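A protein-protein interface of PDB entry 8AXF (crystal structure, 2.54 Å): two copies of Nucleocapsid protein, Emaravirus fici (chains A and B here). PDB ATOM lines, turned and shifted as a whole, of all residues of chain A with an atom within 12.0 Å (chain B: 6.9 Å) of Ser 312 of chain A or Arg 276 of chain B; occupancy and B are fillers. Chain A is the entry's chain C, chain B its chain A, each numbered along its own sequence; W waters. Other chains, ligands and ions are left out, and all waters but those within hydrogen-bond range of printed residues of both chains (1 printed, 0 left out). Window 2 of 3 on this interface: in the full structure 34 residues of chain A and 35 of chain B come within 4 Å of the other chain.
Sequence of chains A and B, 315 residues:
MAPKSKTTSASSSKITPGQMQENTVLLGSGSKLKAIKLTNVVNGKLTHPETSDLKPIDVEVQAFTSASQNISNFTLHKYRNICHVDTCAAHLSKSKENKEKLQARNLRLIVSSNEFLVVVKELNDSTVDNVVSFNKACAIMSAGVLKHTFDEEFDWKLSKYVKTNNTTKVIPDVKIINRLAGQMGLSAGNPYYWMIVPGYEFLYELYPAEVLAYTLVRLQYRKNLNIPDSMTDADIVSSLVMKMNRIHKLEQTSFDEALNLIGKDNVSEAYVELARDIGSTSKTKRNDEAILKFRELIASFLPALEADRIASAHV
Of the printed residues of chain B, Ile 298 of chain A touches Tyr 271 (3.7 Å).
Of the printed residues of chain B, Phe 301 of chain A touches Tyr 271 (3.5 Å).
Printed residues of chain B within 4 Å of Leu 305 of chain A: Tyr 271 (3.9 Å), Val 272 (3.96 Å) and Ala 275 (3.7 Å).
Printed residues of chain B within 4 Å of Asp 308 of chain A: Arg 276 (2.6 Å).
Ser 312 of chain A touches just one residue of chain B: Arg 276.
Of the printed residues of chain A, Tyr 271 of chain B touches Ile 298, Phe 301 and Leu 305.
Of chain A, only Leu 305 (3.96 Å) comes within 4 Å of Val 272 of chain B.
Ala 275 of chain B touches just one residue of chain A: Leu 305 (3.7 Å).
Arg 276 of chain B touches just these residues of chain A: Asp 308 (2.6 Å), Arg 309 (3.3 Å) and Ser 312 (3.9 Å).
Asp 277 of chain B touches none of the printed residues of chain A.
No residue of chain A comes within 4 Å of Gly 279 of chain B.
The nearest printed residue of chain B that does not touch Ile 298 of chain A is Val 272 of chain B (8.4 Å).
The side-chain carboxylate of Glu 306 of chain A lies within salt-bridge range of the guanidinium group of Arg 309 of chain A (2.8 Å).
The side-chain carboxylate (OE2) of Glu 273 of chain B lies within salt-bridge range of the guanidinium group (NH1) of Arg 276 of chain B, 2.9 Å away.
Tyr 271 of chain B touches Ile 298 of chain A (OH to CG2, 3.7 Å).
Phe 301 of chain A touches Tyr 271 of chain B.
Leu 305 of chain A touches Tyr 271 of chain B.
Leu 305 of chain A touches Val 272 of chain B (N to CG1, 3.96 Å).
CB of Ala 275 of chain B touches CD1 of Leu 305 of chain A, at 3.7 Å.
CD of Arg 309 of chain A touches O of Arg 276 of chain B (3.3 Å).
OG of Ser 312 of chain A touches CD of Arg 276 of chain B, at 3.9 Å.
NE of Arg 276 of chain B lies within salt-bridge range of OD1 of Asp 308 of chain A (2.6 Å).
Water W1 lies within hydrogen-bond range of the side-chain hydroxyl (OG) of Ser 312 of chain A (2.8 Å) and the side-chain carboxylate (OD1) of Asp 277 of chain B (3.5 Å).
No position is printed for both chains.
Of the 8 pairs that touch across the chains among the printed residues, none has its exchanged pair printed and touching as well.
Hydrophobic or aromatic side chains of chain B that line the printed part of chain A: Tyr 271, Val 272 and Ala 275.
Of the 14 printed residues of chain A, 6 touch a printed residue of chain B.
Among the printed residues, Asp or Glu carboxylates within 4 Å of a Lys or Arg side-chain nitrogen of the other chain: Asp 308 of chain A with Arg 276 of chain B (2.6 Å).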
ATOM      1  N   ILE A 298       3.234  -0.385 -19.268  1.00  0.00           N
ATOM      2  CA  ILE A 298       3.853  -0.350 -17.945  1.00  0.00           C
ATOM      3  C   ILE A 298       5.119  -1.195 -17.927  1.00  0.00           C
ATOM      4  O   ILE A 298       6.128  -0.817 -17.317  1.00  0.00           O
ATOM      5  CB  ILE A 298       2.842  -0.812 -16.880  1.00  0.00           C
ATOM      6  CG1 ILE A 298       1.759   0.251 -16.676  1.00  0.00           C
ATOM      7  CG2 ILE A 298       3.538  -1.135 -15.567  1.00  0.00           C
ATOM      8  CD1 ILE A 298       0.619  -0.200 -15.784  1.00  0.00           C
ATOM      9  N   PHE A 301       7.979   0.477 -19.704  1.00  0.00           N
ATOM     10  CA  PHE A 301       8.409   1.686 -19.013  1.00  0.00           C
ATOM     11  C   PHE A 301       9.231   1.402 -17.762  1.00  0.00           C
ATOM     12  O   PHE A 301       9.872   2.322 -17.243  1.00  0.00           O
ATOM     13  CB  PHE A 301       7.198   2.542 -18.617  1.00  0.00           C
ATOM     14  CG  PHE A 301       6.439   3.113 -19.783  1.00  0.00           C
ATOM     15  CD1 PHE A 301       7.008   3.172 -21.046  1.00  0.00           C
ATOM     16  CD2 PHE A 301       5.151   3.598 -19.610  1.00  0.00           C
ATOM     17  CE1 PHE A 301       6.304   3.700 -22.113  1.00  0.00           C
ATOM     18  CE2 PHE A 301       4.443   4.128 -20.671  1.00  0.00           C
ATOM     19  CZ  PHE A 301       5.019   4.180 -21.924  1.00  0.00           C
ATOM     20  N   LEU A 302       9.225   0.162 -17.274  1.00  0.00           N
ATOM     21  CA  LEU A 302       9.909  -0.148 -16.021  1.00  0.00           C
ATOM     22  C   LEU A 302      11.410   0.122 -16.047  1.00  0.00           C
ATOM     23  O   LEU A 302      11.926   0.637 -15.039  1.00  0.00           O
ATOM     24  CB  LEU A 302       9.631  -1.606 -15.628  1.00  0.00           C
ATOM     25  CG  LEU A 302      10.281  -2.072 -14.323  1.00  0.00           C
ATOM     26  CD1 LEU A 302       9.818  -1.214 -13.152  1.00  0.00           C
ATOM     27  CD2 LEU A 302       9.996  -3.544 -14.065  1.00  0.00           C
ATOM     28  N   PRO A 303      12.165  -0.205 -17.108  1.00  0.00           N
ATOM     29  CA  PRO A 303      13.599   0.146 -17.099  1.00  0.00           C
ATOM     30  C   PRO A 303      13.863   1.624 -16.868  1.00  0.00           C
ATOM     31  O   PRO A 303      14.619   1.979 -15.954  1.00  0.00           O
ATOM     32  CB  PRO A 303      14.071  -0.313 -18.485  1.00  0.00           C
ATOM     33  CG  PRO A 303      13.174  -1.438 -18.819  1.00  0.00           C
ATOM     34  CD  PRO A 303      11.829  -1.060 -18.264  1.00  0.00           C
ATOM     35  N   ALA A 304      13.257   2.500 -17.675  1.00  0.00           N
ATOM     36  CA  ALA A 304      13.441   3.935 -17.483  1.00  0.00           C
ATOM     37  C   ALA A 304      13.017   4.364 -16.085  1.00  0.00           C
ATOM     38  O   ALA A 304      13.635   5.250 -15.483  1.00  0.00           O
ATOM     39  CB  ALA A 304      12.657   4.711 -18.541  1.00  0.00           C
ATOM     40  N   LEU A 305      11.969   3.736 -15.549  1.00  0.00           N
ATOM     41  CA  LEU A 305      11.504   4.067 -14.206  1.00  0.00           C
ATOM     42  C   LEU A 305      12.572   3.753 -13.164  1.00  0.00           C
ATOM     43  O   LEU A 305      12.997   4.631 -12.408  1.00  0.00           O
ATOM     44  CB  LEU A 305      10.208   3.312 -13.906  1.00  0.00           C
ATOM     45  CG  LEU A 305       9.634   3.465 -12.499  1.00  0.00           C
ATOM     46  CD1 LEU A 305       9.496   4.934 -12.128  1.00  0.00           C
ATOM     47  CD2 LEU A 305       8.293   2.760 -12.409  1.00  0.00           C
ATOM     48  N   GLU A 306      13.024   2.497 -13.116  1.00  0.00           N
ATOM     49  CA  GLU A 306      14.025   2.119 -12.123  1.00  0.00           C
ATOM     50  C   GLU A 306      15.352   2.827 -12.359  1.00  0.00           C
ATOM     51  O   GLU A 306      16.052   3.157 -11.395  1.00  0.00           O
ATOM     52  CB  GLU A 306      14.221   0.604 -12.118  1.00  0.00           C
ATOM     53  CG  GLU A 306      13.061  -0.157 -11.507  1.00  0.00           C
ATOM     54  CD  GLU A 306      12.785   0.257 -10.076  1.00  0.00           C
ATOM     55  OE1 GLU A 306      13.750   0.498  -9.323  1.00  0.00           O
ATOM     56  OE2 GLU A 306      11.597   0.346  -9.704  1.00  0.00           O
ATOM     57  N   ALA A 307      15.716   3.072 -13.619  1.00  0.00           N
ATOM     58  CA  ALA A 307      16.937   3.820 -13.893  1.00  0.00           C
ATOM     59  C   ALA A 307      16.846   5.246 -13.369  1.00  0.00           C
ATOM     60  O   ALA A 307      17.860   5.825 -12.960  1.00  0.00           O
ATOM     61  CB  ALA A 307      17.230   3.826 -15.392  1.00  0.00           C
ATOM     62  N   ASP A 308      15.643   5.826 -13.366  1.00  0.00           N
ATOM     63  CA  ASP A 308      15.486   7.194 -12.885  1.00  0.00           C
ATOM     64  C   ASP A 308      15.551   7.257 -11.364  1.00  0.00           C
ATOM     65  O   ASP A 308      16.102   8.211 -10.801  1.00  0.00           O
ATOM     66  CB  ASP A 308      14.169   7.780 -13.400  1.00  0.00           C
ATOM     67  CG  ASP A 308      14.060   9.280 -13.170  1.00  0.00           C
ATOM     68  OD1 ASP A 308      13.997   9.707 -11.999  1.00  0.00           O
ATOM     69  OD2 ASP A 308      14.040  10.034 -14.168  1.00  0.00           O
ATOM     70  N   ARG A 309      14.999   6.252 -10.678  1.00  0.00           N
ATOM     71  CA  ARG A 309      14.948   6.311  -9.220  1.00  0.00           C
ATOM     72  C   ARG A 309      16.332   6.124  -8.607  1.00  0.00           C
ATOM     73  O   ARG A 309      16.639   6.719  -7.568  1.00  0.00           O
ATOM     74  CB  ARG A 309      13.976   5.265  -8.673  1.00  0.00           C
ATOM     75  CG  ARG A 309      12.605   5.237  -9.336  1.00  0.00           C
ATOM     76  CD  ARG A 309      11.618   4.457  -8.474  1.00  0.00           C
ATOM     77  NE  ARG A 309      10.815   3.497  -9.229  1.00  0.00           N
ATOM     78  CZ  ARG A 309       9.948   2.658  -8.672  1.00  0.00           C
ATOM     79  NH1 ARG A 309       9.776   2.659  -7.358  1.00  0.00           N
ATOM     80  NH2 ARG A 309       9.256   1.810  -9.422  1.00  0.00           N
ATOM     81  N   ILE A 310      17.180   5.303  -9.229  1.00  0.00           N
ATOM     82  CA  ILE A 310      18.540   5.168  -8.724  1.00  0.00           C
ATOM     83  C   ILE A 310      19.317   6.455  -8.946  1.00  0.00           C
ATOM     84  O   ILE A 310      20.228   6.781  -8.176  1.00  0.00           O
ATOM     85  CB  ILE A 310      19.250   3.972  -9.378  1.00  0.00           C
ATOM     86  CG1 ILE A 310      18.334   2.747  -9.377  1.00  0.00           C
ATOM     87  CG2 ILE A 310      20.553   3.685  -8.651  1.00  0.00           C
ATOM     88  CD1 ILE A 310      18.133   2.128  -8.023  1.00  0.00           C
ATOM     89  N   ALA A 311      18.980   7.206  -9.997  1.00  0.00           N
ATOM     90  CA  ALA A 311      19.624   8.491 -10.237  1.00  0.00           C
ATOM     91  C   ALA A 311      19.035   9.593  -9.367  1.00  0.00           C
ATOM     92  O   ALA A 311      19.729  10.567  -9.055  1.00  0.00           O
ATOM     93  CB  ALA A 311      19.509   8.866 -11.715  1.00  0.00           C
ATOM     94  N   SER A 312      17.771   9.461  -8.973  1.00  0.00           N
ATOM     95  CA  SER A 312      17.127  10.431  -8.102  1.00  0.00           C
ATOM     96  C   SER A 312      17.600  10.260  -6.661  1.00  0.00           C
ATOM     97  O   SER A 312      18.140   9.220  -6.276  1.00  0.00           O
ATOM     98  CB  SER A 312      15.605  10.290  -8.172  1.00  0.00           C
ATOM     99  OG  SER A 312      14.998  10.719  -6.964  1.00  0.00           O
ATOM    100  N   ALA A 313      17.381  11.302  -5.863  1.00  0.00           N
ATOM    101  CA  ALA A 313      17.824  11.333  -4.470  1.00  0.00           C
ATOM    102  C   ALA A 313      17.250  10.176  -3.656  1.00  0.00           C
ATOM    103  O   ALA A 313      17.996   9.379  -3.084  1.00  0.00           O
ATOM    104  CB  ALA A 313      17.449  12.662  -3.828  1.00  0.00           C
ATOM    105  N   MET B 184       0.801  10.059  -3.747  1.00  0.00           N
ATOM    106  CA  MET B 184       1.722   9.584  -4.769  1.00  0.00           C
ATOM    107  C   MET B 184       3.171   9.953  -4.486  1.00  0.00           C
ATOM    108  O   MET B 184       4.060   9.529  -5.234  1.00  0.00           O
ATOM    109  CB  MET B 184       1.339  10.149  -6.140  1.00  0.00           C
ATOM    110  CG  MET B 184      -0.080   9.857  -6.582  1.00  0.00           C
ATOM    111  SD  MET B 184      -0.395  10.530  -8.224  1.00  0.00           S
ATOM    112  CE  MET B 184       0.943   9.782  -9.150  1.00  0.00           C
ATOM    113  N   LEU B 186       4.194  13.071  -4.699  1.00  0.00           N
ATOM    114  CA  LEU B 186       4.432  14.360  -5.331  1.00  0.00           C
ATOM    115  C   LEU B 186       4.393  15.469  -4.288  1.00  0.00           C
ATOM    116  O   LEU B 186       3.599  15.429  -3.344  1.00  0.00           O
ATOM    117  CB  LEU B 186       3.389  14.629  -6.417  1.00  0.00           C
ATOM    118  CG  LEU B 186       3.257  13.638  -7.575  1.00  0.00           C
ATOM    119  CD1 LEU B 186       2.281  14.168  -8.620  1.00  0.00           C
ATOM    120  CD2 LEU B 186       4.609  13.345  -8.202  1.00  0.00           C
ATOM    121  N   ASN B 190       5.384  20.792  -8.160  1.00  0.00           N
ATOM    122  CA  ASN B 190       5.473  19.891  -9.300  1.00  0.00           C
ATOM    123  C   ASN B 190       4.422  20.289 -10.332  1.00  0.00           C
ATOM    124  O   ASN B 190       3.264  20.517  -9.969  1.00  0.00           O
ATOM    125  CB  ASN B 190       5.262  18.452  -8.829  1.00  0.00           C
ATOM    126  CG  ASN B 190       5.689  17.422  -9.857  1.00  0.00           C
ATOM    127  OD1 ASN B 190       5.353  17.524 -11.035  1.00  0.00           O
ATOM    128  ND2 ASN B 190       6.433  16.415  -9.408  1.00  0.00           N
ATOM    129  N   GLU B 269       7.744   9.548 -20.349  1.00  0.00           N
ATOM    130  CA  GLU B 269       8.319  10.594 -19.507  1.00  0.00           C
ATOM    131  C   GLU B 269       7.352  11.012 -18.410  1.00  0.00           C
ATOM    132  O   GLU B 269       7.748  11.172 -17.249  1.00  0.00           O
ATOM    133  CB  GLU B 269       8.699  11.805 -20.356  1.00  0.00           C
ATOM    134  CG  GLU B 269       9.650  11.497 -21.491  1.00  0.00           C
ATOM    135  CD  GLU B 269       9.761  12.640 -22.477  1.00  0.00           C
ATOM    136  OE1 GLU B 269       8.935  13.575 -22.400  1.00  0.00           O
ATOM    137  OE2 GLU B 269      10.673  12.602 -23.329  1.00  0.00           O
ATOM    138  N   ALA B 270       6.081  11.208 -18.763  1.00  0.00           N
ATOM    139  CA  ALA B 270       5.074  11.528 -17.760  1.00  0.00           C
ATOM    140  C   ALA B 270       4.921  10.390 -16.761  1.00  0.00           C
ATOM    141  O   ALA B 270       4.762  10.628 -15.557  1.00  0.00           O
ATOM    142  CB  ALA B 270       3.741  11.837 -18.441  1.00  0.00           C
ATOM    143  N   TYR B 271       4.978   9.145 -17.239  1.00  0.00           N
ATOM    144  CA  TYR B 271       4.858   8.000 -16.343  1.00  0.00           C
ATOM    145  C   TYR B 271       5.967   8.002 -15.297  1.00  0.00           C
ATOM    146  O   TYR B 271       5.707   7.830 -14.102  1.00  0.00           O
ATOM    147  CB  TYR B 271       4.871   6.696 -17.143  1.00  0.00           C
ATOM    148  CG  TYR B 271       4.777   5.454 -16.284  1.00  0.00           C
ATOM    149  CD1 TYR B 271       3.589   5.110 -15.656  1.00  0.00           C
ATOM    150  CD2 TYR B 271       5.878   4.621 -16.105  1.00  0.00           C
ATOM    151  CE1 TYR B 271       3.495   3.977 -14.868  1.00  0.00           C
ATOM    152  CE2 TYR B 271       5.793   3.482 -15.319  1.00  0.00           C
ATOM    153  CZ  TYR B 271       4.600   3.167 -14.703  1.00  0.00           C
ATOM    154  OH  TYR B 271       4.508   2.037 -13.921  1.00  0.00           O
ATOM    155  N   VAL B 272       7.214   8.210 -15.728  1.00  0.00           N
ATOM    156  CA  VAL B 272       8.315   8.164 -14.772  1.00  0.00           C
ATOM    157  C   VAL B 272       8.309   9.397 -13.877  1.00  0.00           C
ATOM    158  O   VAL B 272       8.815   9.352 -12.750  1.00  0.00           O
ATOM    159  CB  VAL B 272       9.666   7.989 -15.497  1.00  0.00           C
ATOM    160  CG1 VAL B 272       9.617   6.793 -16.435  1.00  0.00           C
ATOM    161  CG2 VAL B 272      10.050   9.247 -16.249  1.00  0.00           C
ATOM    162  N   GLU B 273       7.742  10.511 -14.348  1.00  0.00           N
ATOM    163  CA  GLU B 273       7.578  11.671 -13.475  1.00  0.00           C
ATOM    164  C   GLU B 273       6.587  11.370 -12.359  1.00  0.00           C
ATOM    165  O   GLU B 273       6.836  11.684 -11.188  1.00  0.00           O
ATOM    166  CB  GLU B 273       7.120  12.889 -14.280  1.00  0.00           C
ATOM    167  CG  GLU B 273       8.212  13.581 -15.081  1.00  0.00           C
ATOM    168  CD  GLU B 273       9.358  14.074 -14.214  1.00  0.00           C
ATOM    169  OE1 GLU B 273      10.500  14.127 -14.714  1.00  0.00           O
ATOM    170  OE2 GLU B 273       9.119  14.407 -13.033  1.00  0.00           O
ATOM    171  N   LEU B 274       5.458  10.752 -12.705  1.00  0.00           N
ATOM    172  CA  LEU B 274       4.419  10.455 -11.730  1.00  0.00           C
ATOM    173  C   LEU B 274       4.731   9.225 -10.887  1.00  0.00           C
ATOM    174  O   LEU B 274       4.194   9.098  -9.781  1.00  0.00           O
ATOM    175  CB  LEU B 274       3.081  10.270 -12.448  1.00  0.00           C
ATOM    176  CG  LEU B 274       2.542  11.539 -13.114  1.00  0.00           C
ATOM    177  CD1 LEU B 274       1.664  11.200 -14.306  1.00  0.00           C
ATOM    178  CD2 LEU B 274       1.773  12.373 -12.103  1.00  0.00           C
ATOM    179  N   ALA B 275       5.586   8.327 -11.371  1.00  0.00           N
ATOM    180  CA  ALA B 275       5.887   7.096 -10.653  1.00  0.00           C
ATOM    181  C   ALA B 275       7.153   7.175  -9.813  1.00  0.00           C
ATOM    182  O   ALA B 275       7.362   6.303  -8.964  1.00  0.00           O
ATOM    183  CB  ALA B 275       6.013   5.924 -11.633  1.00  0.00           C
ATOM    184  N   ARG B 276       7.981   8.207 -10.011  1.00  0.00           N
ATOM    185  CA  ARG B 276       9.329   8.221  -9.450  1.00  0.00           C
ATOM    186  C   ARG B 276       9.324   8.006  -7.940  1.00  0.00           C
ATOM    187  O   ARG B 276      10.083   7.179  -7.419  1.00  0.00           O
ATOM    188  CB  ARG B 276      10.024   9.540  -9.792  1.00  0.00           C
ATOM    189  CG  ARG B 276      11.312   9.767  -9.020  1.00  0.00           C
ATOM    190  CD  ARG B 276      11.964  11.092  -9.375  1.00  0.00           C
ATOM    191  NE  ARG B 276      12.217  11.214 -10.808  1.00  0.00           N
ATOM    192  CZ  ARG B 276      11.571  12.050 -11.614  1.00  0.00           C
ATOM    193  NH1 ARG B 276      10.635  12.853 -11.127  1.00  0.00           N
ATOM    194  NH2 ARG B 276      11.867  12.091 -12.905  1.00  0.00           N
ATOM    195  N   ASP B 277       8.476   8.736  -7.218  1.00  0.00           N
ATOM    196  CA  ASP B 277       8.534   8.767  -5.762  1.00  0.00           C
ATOM    197  C   ASP B 277       7.426   7.955  -5.100  1.00  0.00           C
ATOM    198  O   ASP B 277       7.101   8.204  -3.934  1.00  0.00           O
ATOM    199  CB  ASP B 277       8.501  10.213  -5.266  1.00  0.00           C
ATOM    200  CG  ASP B 277       9.841  10.909  -5.418  1.00  0.00           C
ATOM    201  OD1 ASP B 277      10.877  10.272  -5.134  1.00  0.00           O
ATOM    202  OD2 ASP B 277       9.860  12.089  -5.825  1.00  0.00           O
ATOM    203  N   ILE B 278       6.846   6.986  -5.808  1.00  0.00           N
ATOM    204  CA  ILE B 278       5.894   6.082  -5.178  1.00  0.00           C
ATOM    205  C   ILE B 278       6.641   5.138  -4.248  1.00  0.00           C
ATOM    206  O   ILE B 278       7.751   4.680  -4.555  1.00  0.00           O
ATOM    207  CB  ILE B 278       5.101   5.302  -6.239  1.00  0.00           C
ATOM    208  CG1 ILE B 278       4.559   6.254  -7.298  1.00  0.00           C
ATOM    209  CG2 ILE B 278       3.950   4.539  -5.596  1.00  0.00           C
ATOM    210  CD1 ILE B 278       3.737   5.563  -8.335  1.00  0.00           C
ATOM    211  N   GLY B 279       6.039   4.847  -3.100  1.00  0.00           N
ATOM    212  CA  GLY B 279       6.703   4.010  -2.127  1.00  0.00           C
ATOM    213  C   GLY B 279       7.879   4.646  -1.424  1.00  0.00           C
ATOM    214  O   GLY B 279       8.604   3.943  -0.716  1.00  0.00           O
ATOM    215  N   SER B 280       8.099   5.952  -1.595  1.00  0.00           N
ATOM    216  CA  SER B 280       9.219   6.600  -0.919  1.00  0.00           C
ATOM    217  C   SER B 280       9.057   6.512   0.592  1.00  0.00           C
ATOM    218  O   SER B 280       9.985   6.121   1.310  1.00  0.00           O
ATOM    219  CB  SER B 280       9.338   8.055  -1.364  1.00  0.00           C
ATOM    220  OG  SER B 280       8.596   8.896  -0.502  1.00  0.00           O
HETATM  221  O   HOH W   1      13.631   8.390  -6.111  1.00  0.00           O
